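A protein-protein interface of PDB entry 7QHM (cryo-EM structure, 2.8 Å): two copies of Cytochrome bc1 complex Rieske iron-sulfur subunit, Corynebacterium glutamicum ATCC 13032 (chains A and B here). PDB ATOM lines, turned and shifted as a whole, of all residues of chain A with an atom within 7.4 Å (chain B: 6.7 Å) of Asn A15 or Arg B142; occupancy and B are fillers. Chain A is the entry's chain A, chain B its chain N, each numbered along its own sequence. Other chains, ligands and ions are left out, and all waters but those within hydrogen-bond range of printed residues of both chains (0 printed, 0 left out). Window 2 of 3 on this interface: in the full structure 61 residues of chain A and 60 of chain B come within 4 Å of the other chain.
Of the 13 printed residues of chain A, 7 touch a printed residue of chain B. Hydrophobic or aromatic side chains of chain A that line the printed part of chain B: Leu A14 and Leu A22. Of the 11 printed residues of chain B, 6 touch a printed residue of chain A. Printed residues of chain B that touch a printed residue of chain A: Glu B138, Val B139, Arg B142, Thr B143, Ala B146 and Leu B147.
The backbone carbonyl oxygen (O) of Val B139 sits at hydrogen-bond distance from the side-chain hydroxyl (OG1) of Thr B143 (2.6 Å). O of Thr A11 sits close to OD1 of Asn A15 (3.1 Å). O of Asp B140 is in hydrogen-bond range of OG1 of Thr B143, at 2.9 Å.
No position is printed for both chains. Of the 12 pairs that touch across the chains among the printed residues, none has its exchanged pair printed and touching as well.
The side-chain carboxylate of Glu B138 lies within hydrogen-bond range of the side-chain hydroxyl of Thr A11 (2.9 Å). The side-chain amide oxygen (OD1) of Asn A15 is in hydrogen-bond range of the guanidinium group (NH1) of Arg B142, 2.7 Å away. O of Leu A14 is in hydrogen-bond range of NH1 of Arg B142, at 3.4 Å.
Asn A15 touches one residue of chain B. Of the printed residues of chain B, Asn A19 touches Ala B146. Printed residues of chain B within 4 Å of Ala A23: Ala B146 (3.7 Å) and Leu B147 (3.6 Å). Printed residues of chain B within 4 Å of Gly A26: Thr B143. Of the printed residues of chain A, Glu B138 touches Thr A11 (2.9 Å). Of the printed residues of chain A, Arg B142 touches Thr A11 (3.98 Å), Leu A14 (3.4 Å), Asn A15 (2.7 Å) and Leu A22 (3.7 Å). The nearest residue of chain B that does not touch Asn A15 is Glu B138 (6.4 Å). The nearest printed residue of chain A that does not touch Val B139 is Leu A22 (5.7 Å).
Among the printed residues, pairs that only touch across the chains: Ala A23 with Leu B147 (3.6 Å), Leu A22 with Thr B143 (3.6 Å), Leu A22 with Ala B146 (3.6 Å), Leu A22 with Arg B142 (3.7 Å), Asn A19 with Ala B146 (3.7 Å), Ala A23 with Ala B146 (3.7 Å), Gly A26 with Thr B143 (3.8 Å), Leu A14 with Val B139 (3.8 Å) and Thr A11 with Arg B142 (3.98 Å).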
ATOM      1  N   THR A  10      -4.592  10.143 -27.319  1.00  0.00           N
ATOM      2  CA  THR A  10      -5.210   8.852 -27.571  1.00  0.00           C
ATOM      3  C   THR A  10      -6.607   8.820 -26.963  1.00  0.00           C
ATOM      4  O   THR A  10      -6.968   9.655 -26.133  1.00  0.00           O
ATOM      5  CB  THR A  10      -4.355   7.707 -27.020  1.00  0.00           C
ATOM      6  OG1 THR A  10      -4.978   6.454 -27.326  1.00  0.00           O
ATOM      7  CG2 THR A  10      -4.154   7.804 -25.522  1.00  0.00           C
ATOM      8  N   THR A  11      -7.408   7.853 -27.412  1.00  0.00           N
ATOM      9  CA  THR A  11      -8.789   7.776 -26.953  1.00  0.00           C
ATOM     10  C   THR A  11      -8.862   7.552 -25.451  1.00  0.00           C
ATOM     11  O   THR A  11      -9.809   8.008 -24.799  1.00  0.00           O
ATOM     12  CB  THR A  11      -9.518   6.655 -27.695  1.00  0.00           C
ATOM     13  OG1 THR A  11      -9.387   6.854 -29.108  1.00  0.00           O
ATOM     14  CG2 THR A  11     -11.001   6.624 -27.330  1.00  0.00           C
ATOM     15  N   GLN A  12      -7.875   6.855 -24.889  1.00  0.00           N
ATOM     16  CA  GLN A  12      -7.863   6.610 -23.453  1.00  0.00           C
ATOM     17  C   GLN A  12      -7.629   7.897 -22.676  1.00  0.00           C
ATOM     18  O   GLN A  12      -8.218   8.097 -21.608  1.00  0.00           O
ATOM     19  CB  GLN A  12      -6.793   5.575 -23.124  1.00  0.00           C
ATOM     20  CG  GLN A  12      -6.751   5.150 -21.667  1.00  0.00           C
ATOM     21  CD  GLN A  12      -5.831   3.967 -21.441  1.00  0.00           C
ATOM     22  OE1 GLN A  12      -5.243   3.435 -22.383  1.00  0.00           O
ATOM     23  NE2 GLN A  12      -5.701   3.549 -20.190  1.00  0.00           N
ATOM     24  N   GLU A  13      -6.779   8.786 -23.192  1.00  0.00           N
ATOM     25  CA  GLU A  13      -6.498  10.021 -22.470  1.00  0.00           C
ATOM     26  C   GLU A  13      -7.676  10.975 -22.545  1.00  0.00           C
ATOM     27  O   GLU A  13      -8.026  11.612 -21.545  1.00  0.00           O
ATOM     28  CB  GLU A  13      -5.237  10.684 -23.020  1.00  0.00           C
ATOM     29  CG  GLU A  13      -3.952   9.925 -22.702  1.00  0.00           C
ATOM     30  CD  GLU A  13      -3.607   9.938 -21.222  1.00  0.00           C
ATOM     31  OE1 GLU A  13      -3.604  11.029 -20.616  1.00  0.00           O
ATOM     32  OE2 GLU A  13      -3.352   8.851 -20.663  1.00  0.00           O
ATOM     33  N   LEU A  14      -8.301  11.089 -23.715  1.00  0.00           N
ATOM     34  CA  LEU A  14      -9.506  11.897 -23.820  1.00  0.00           C
ATOM     35  C   LEU A  14     -10.612  11.352 -22.932  1.00  0.00           C
ATOM     36  O   LEU A  14     -11.429  12.123 -22.417  1.00  0.00           O
ATOM     37  CB  LEU A  14      -9.970  11.959 -25.273  1.00  0.00           C
ATOM     38  CG  LEU A  14      -9.029  12.622 -26.282  1.00  0.00           C
ATOM     39  CD1 LEU A  14      -9.542  12.400 -27.681  1.00  0.00           C
ATOM     40  CD2 LEU A  14      -8.898  14.103 -26.010  1.00  0.00           C
ATOM     41  N   ASN A  15     -10.649  10.034 -22.726  1.00  0.00           N
ATOM     42  CA  ASN A  15     -11.629   9.461 -21.809  1.00  0.00           C
ATOM     43  C   ASN A  15     -11.294   9.793 -20.363  1.00  0.00           C
ATOM     44  O   ASN A  15     -12.197  10.006 -19.545  1.00  0.00           O
ATOM     45  CB  ASN A  15     -11.706   7.949 -21.997  1.00  0.00           C
ATOM     46  CG  ASN A  15     -12.439   7.561 -23.247  1.00  0.00           C
ATOM     47  OD1 ASN A  15     -12.831   8.413 -24.035  1.00  0.00           O
ATOM     48  ND2 ASN A  15     -12.631   6.262 -23.440  1.00  0.00           N
ATOM     49  N   ALA A  16     -10.007   9.844 -20.027  1.00  0.00           N
ATOM     50  CA  ALA A  16      -9.613  10.116 -18.651  1.00  0.00           C
ATOM     51  C   ALA A  16     -10.009  11.514 -18.186  1.00  0.00           C
ATOM     52  O   ALA A  16     -10.055  11.759 -16.976  1.00  0.00           O
ATOM     53  CB  ALA A  16      -8.102   9.935 -18.501  1.00  0.00           C
ATOM     54  N   MET A  17     -10.298  12.430 -19.106  1.00  0.00           N
ATOM     55  CA  MET A  17     -10.545  13.816 -18.751  1.00  0.00           C
ATOM     56  C   MET A  17     -11.975  14.019 -18.260  1.00  0.00           C
ATOM     57  O   MET A  17     -12.878  13.222 -18.530  1.00  0.00           O
ATOM     58  CB  MET A  17     -10.288  14.725 -19.951  1.00  0.00           C
ATOM     59  CG  MET A  17      -8.854  14.735 -20.414  1.00  0.00           C
ATOM     60  SD  MET A  17      -8.631  15.633 -21.947  1.00  0.00           S
ATOM     61  CE  MET A  17      -7.080  14.940 -22.503  1.00  0.00           C
ATOM     62  N   SER A  18     -12.164  15.109 -17.525  1.00  0.00           N
ATOM     63  CA  SER A  18     -13.484  15.604 -17.173  1.00  0.00           C
ATOM     64  C   SER A  18     -13.976  16.551 -18.256  1.00  0.00           C
ATOM     65  O   SER A  18     -13.211  17.017 -19.099  1.00  0.00           O
ATOM     66  CB  SER A  18     -13.458  16.318 -15.825  1.00  0.00           C
ATOM     67  OG  SER A  18     -14.716  16.909 -15.544  1.00  0.00           O
ATOM     68  N   ASN A  19     -15.276  16.833 -18.227  1.00  0.00           N
ATOM     69  CA  ASN A  19     -15.883  17.580 -19.325  1.00  0.00           C
ATOM     70  C   ASN A  19     -15.387  19.021 -19.355  1.00  0.00           C
ATOM     71  O   ASN A  19     -15.171  19.588 -20.435  1.00  0.00           O
ATOM     72  CB  ASN A  19     -17.407  17.522 -19.207  1.00  0.00           C
ATOM     73  CG  ASN A  19     -18.103  17.630 -20.547  1.00  0.00           C
ATOM     74  OD1 ASN A  19     -18.867  18.563 -20.789  1.00  0.00           O
ATOM     75  ND2 ASN A  19     -17.842  16.670 -21.430  1.00  0.00           N
ATOM     76  N   LEU A  22     -11.941  18.952 -20.992  1.00  0.00           N
ATOM     77  CA  LEU A  22     -12.097  18.897 -22.439  1.00  0.00           C
ATOM     78  C   LEU A  22     -12.495  20.251 -23.001  1.00  0.00           C
ATOM     79  O   LEU A  22     -12.046  20.635 -24.083  1.00  0.00           O
ATOM     80  CB  LEU A  22     -13.136  17.846 -22.811  1.00  0.00           C
ATOM     81  CG  LEU A  22     -12.662  16.398 -22.787  1.00  0.00           C
ATOM     82  CD1 LEU A  22     -13.842  15.469 -22.686  1.00  0.00           C
ATOM     83  CD2 LEU A  22     -11.849  16.074 -24.018  1.00  0.00           C
ATOM     84  N   ALA A  23     -13.325  21.002 -22.276  1.00  0.00           N
ATOM     85  CA  ALA A  23     -13.683  22.336 -22.745  1.00  0.00           C
ATOM     86  C   ALA A  23     -12.477  23.268 -22.745  1.00  0.00           C
ATOM     87  O   ALA A  23     -12.290  24.051 -23.685  1.00  0.00           O
ATOM     88  CB  ALA A  23     -14.805  22.910 -21.886  1.00  0.00           C
ATOM     89  N   GLY A  26     -10.468  22.506 -25.593  1.00  0.00           N
ATOM     90  CA  GLY A  26     -11.134  22.977 -26.794  1.00  0.00           C
ATOM     91  C   GLY A  26     -10.877  24.442 -27.079  1.00  0.00           C
ATOM     92  O   GLY A  26     -10.597  24.822 -28.218  1.00  0.00           O
ATOM     93  N   GLU B 137     -11.243  14.213 -36.507  1.00  0.00           N
ATOM     94  CA  GLU B 137     -10.494  13.512 -35.484  1.00  0.00           C
ATOM     95  C   GLU B 137     -11.307  13.498 -34.195  1.00  0.00           C
ATOM     96  O   GLU B 137     -12.210  14.311 -33.994  1.00  0.00           O
ATOM     97  CB  GLU B 137      -9.129  14.169 -35.276  1.00  0.00           C
ATOM     98  CG  GLU B 137      -8.168  13.417 -34.357  1.00  0.00           C
ATOM     99  CD  GLU B 137      -7.920  11.977 -34.782  1.00  0.00           C
ATOM    100  OE1 GLU B 137      -8.802  11.123 -34.553  1.00  0.00           O
ATOM    101  OE2 GLU B 137      -6.846  11.702 -35.353  1.00  0.00           O
ATOM    102  N   GLU B 138     -11.000  12.537 -33.323  1.00  0.00           N
ATOM    103  CA  GLU B 138     -11.844  12.343 -32.152  1.00  0.00           C
ATOM    104  C   GLU B 138     -11.711  13.484 -31.159  1.00  0.00           C
ATOM    105  O   GLU B 138     -12.668  13.788 -30.444  1.00  0.00           O
ATOM    106  CB  GLU B 138     -11.517  11.018 -31.474  1.00  0.00           C
ATOM    107  CG  GLU B 138     -12.225   9.832 -32.095  1.00  0.00           C
ATOM    108  CD  GLU B 138     -11.881   8.525 -31.409  1.00  0.00           C
ATOM    109  OE1 GLU B 138     -11.342   8.565 -30.283  1.00  0.00           O
ATOM    110  OE2 GLU B 138     -12.149   7.457 -31.998  1.00  0.00           O
ATOM    111  N   VAL B 139     -10.541  14.117 -31.086  1.00  0.00           N
ATOM    112  CA  VAL B 139     -10.369  15.206 -30.134  1.00  0.00           C
ATOM    113  C   VAL B 139     -11.266  16.381 -30.502  1.00  0.00           C
ATOM    114  O   VAL B 139     -11.845  17.033 -29.629  1.00  0.00           O
ATOM    115  CB  VAL B 139      -8.886  15.612 -30.036  1.00  0.00           C
ATOM    116  CG1 VAL B 139      -8.328  16.082 -31.380  1.00  0.00           C
ATOM    117  CG2 VAL B 139      -8.696  16.683 -28.965  1.00  0.00           C
ATOM    118  N   ASP B 140     -11.418  16.658 -31.795  1.00  0.00           N
ATOM    119  CA  ASP B 140     -12.273  17.763 -32.211  1.00  0.00           C
ATOM    120  C   ASP B 140     -13.729  17.492 -31.866  1.00  0.00           C
ATOM    121  O   ASP B 140     -14.437  18.381 -31.376  1.00  0.00           O
ATOM    122  CB  ASP B 140     -12.106  18.004 -33.704  1.00  0.00           C
ATOM    123  CG  ASP B 140     -10.757  18.580 -34.042  1.00  0.00           C
ATOM    124  OD1 ASP B 140     -10.348  19.555 -33.378  1.00  0.00           O
ATOM    125  OD2 ASP B 140     -10.094  18.055 -34.961  1.00  0.00           O
ATOM    126  N   ARG B 141     -14.185  16.266 -32.101  1.00  0.00           N
ATOM    127  CA  ARG B 141     -15.552  15.896 -31.773  1.00  0.00           C
ATOM    128  C   ARG B 141     -15.792  15.994 -30.274  1.00  0.00           C
ATOM    129  O   ARG B 141     -16.776  16.596 -29.817  1.00  0.00           O
ATOM    130  CB  ARG B 141     -15.821  14.481 -32.286  1.00  0.00           C
ATOM    131  CG  ARG B 141     -15.701  14.332 -33.801  1.00  0.00           C
ATOM    132  CD  ARG B 141     -15.508  12.892 -34.224  1.00  0.00           C
ATOM    133  NE  ARG B 141     -16.645  12.046 -33.884  1.00  0.00           N
ATOM    134  CZ  ARG B 141     -17.698  11.816 -34.659  1.00  0.00           C
ATOM    135  NH1 ARG B 141     -17.829  12.378 -35.849  1.00  0.00           N
ATOM    136  NH2 ARG B 141     -18.647  10.993 -34.230  1.00  0.00           N
ATOM    137  N   ARG B 142     -14.879  15.432 -29.486  1.00  0.00           N
ATOM    138  CA  ARG B 142     -15.035  15.460 -28.039  1.00  0.00           C
ATOM    139  C   ARG B 142     -14.991  16.886 -27.507  1.00  0.00           C
ATOM    140  O   ARG B 142     -15.803  17.260 -26.653  1.00  0.00           O
ATOM    141  CB  ARG B 142     -13.949  14.607 -27.392  1.00  0.00           C
ATOM    142  CG  ARG B 142     -14.325  14.082 -26.029  1.00  0.00           C
ATOM    143  CD  ARG B 142     -15.224  12.876 -26.127  1.00  0.00           C
ATOM    144  NE  ARG B 142     -14.512  11.720 -26.658  1.00  0.00           N
ATOM    145  CZ  ARG B 142     -13.827  10.842 -25.936  1.00  0.00           C
ATOM    146  NH1 ARG B 142     -13.732  10.941 -24.620  1.00  0.00           N
ATOM    147  NH2 ARG B 142     -13.222   9.834 -26.554  1.00  0.00           N
ATOM    148  N   THR B 143     -14.074  17.707 -28.022  1.00  0.00           N
ATOM    149  CA  THR B 143     -13.945  19.070 -27.515  1.00  0.00           C
ATOM    150  C   THR B 143     -15.142  19.933 -27.892  1.00  0.00           C
ATOM    151  O   THR B 143     -15.590  20.756 -27.086  1.00  0.00           O
ATOM    152  CB  THR B 143     -12.661  19.711 -28.024  1.00  0.00           C
ATOM    153  OG1 THR B 143     -12.542  19.503 -29.434  1.00  0.00           O
ATOM    154  CG2 THR B 143     -11.460  19.119 -27.310  1.00  0.00           C
ATOM    155  N   ILE B 144     -15.680  19.779 -29.105  1.00  0.00           N
ATOM    156  CA  ILE B 144     -16.824  20.608 -29.462  1.00  0.00           C
ATOM    157  C   ILE B 144     -18.049  20.180 -28.668  1.00  0.00           C
ATOM    158  O   ILE B 144     -18.865  21.019 -28.265  1.00  0.00           O
ATOM    159  CB  ILE B 144     -17.082  20.595 -30.985  1.00  0.00           C
ATOM    160  CG1 ILE B 144     -18.112  21.669 -31.347  1.00  0.00           C
ATOM    161  CG2 ILE B 144     -17.561  19.250 -31.473  1.00  0.00           C
ATOM    162  CD1 ILE B 144     -18.160  22.016 -32.810  1.00  0.00           C
ATOM    163  N   VAL B 145     -18.190  18.879 -28.405  1.00  0.00           N
ATOM    164  CA  VAL B 145     -19.306  18.444 -27.574  1.00  0.00           C
ATOM    165  C   VAL B 145     -19.148  18.984 -26.163  1.00  0.00           C
ATOM    166  O   VAL B 145     -20.130  19.370 -25.520  1.00  0.00           O
ATOM    167  CB  VAL B 145     -19.420  16.912 -27.589  1.00  0.00           C
ATOM    168  CG1 VAL B 145     -20.382  16.438 -26.532  1.00  0.00           C
ATOM    169  CG2 VAL B 145     -19.874  16.440 -28.946  1.00  0.00           C
ATOM    170  N   ALA B 146     -17.914  19.030 -25.661  1.00  0.00           N
ATOM    171  CA  ALA B 146     -17.682  19.585 -24.334  1.00  0.00           C
ATOM    172  C   ALA B 146     -18.041  21.058 -24.291  1.00  0.00           C
ATOM    173  O   ALA B 146     -18.645  21.527 -23.326  1.00  0.00           O
ATOM    174  CB  ALA B 146     -16.226  19.391 -23.930  1.00  0.00           C
ATOM    175  N   LEU B 147     -17.691  21.806 -25.334  1.00  0.00           N
ATOM    176  CA  LEU B 147     -17.982  23.234 -25.329  1.00  0.00           C
ATOM    177  C   LEU B 147     -19.478  23.496 -25.412  1.00  0.00           C
ATOM    178  O   LEU B 147     -19.991  24.395 -24.737  1.00  0.00           O
ATOM    179  CB  LEU B 147     -17.244  23.925 -26.475  1.00  0.00           C
ATOM    180  CG  LEU B 147     -15.729  24.006 -26.308  1.00  0.00           C
ATOM    181  CD1 LEU B 147     -15.057  24.335 -27.618  1.00  0.00           C
ATOM    182  CD2 LEU B 147     -15.352  25.038 -25.274  1.00  0.00           C
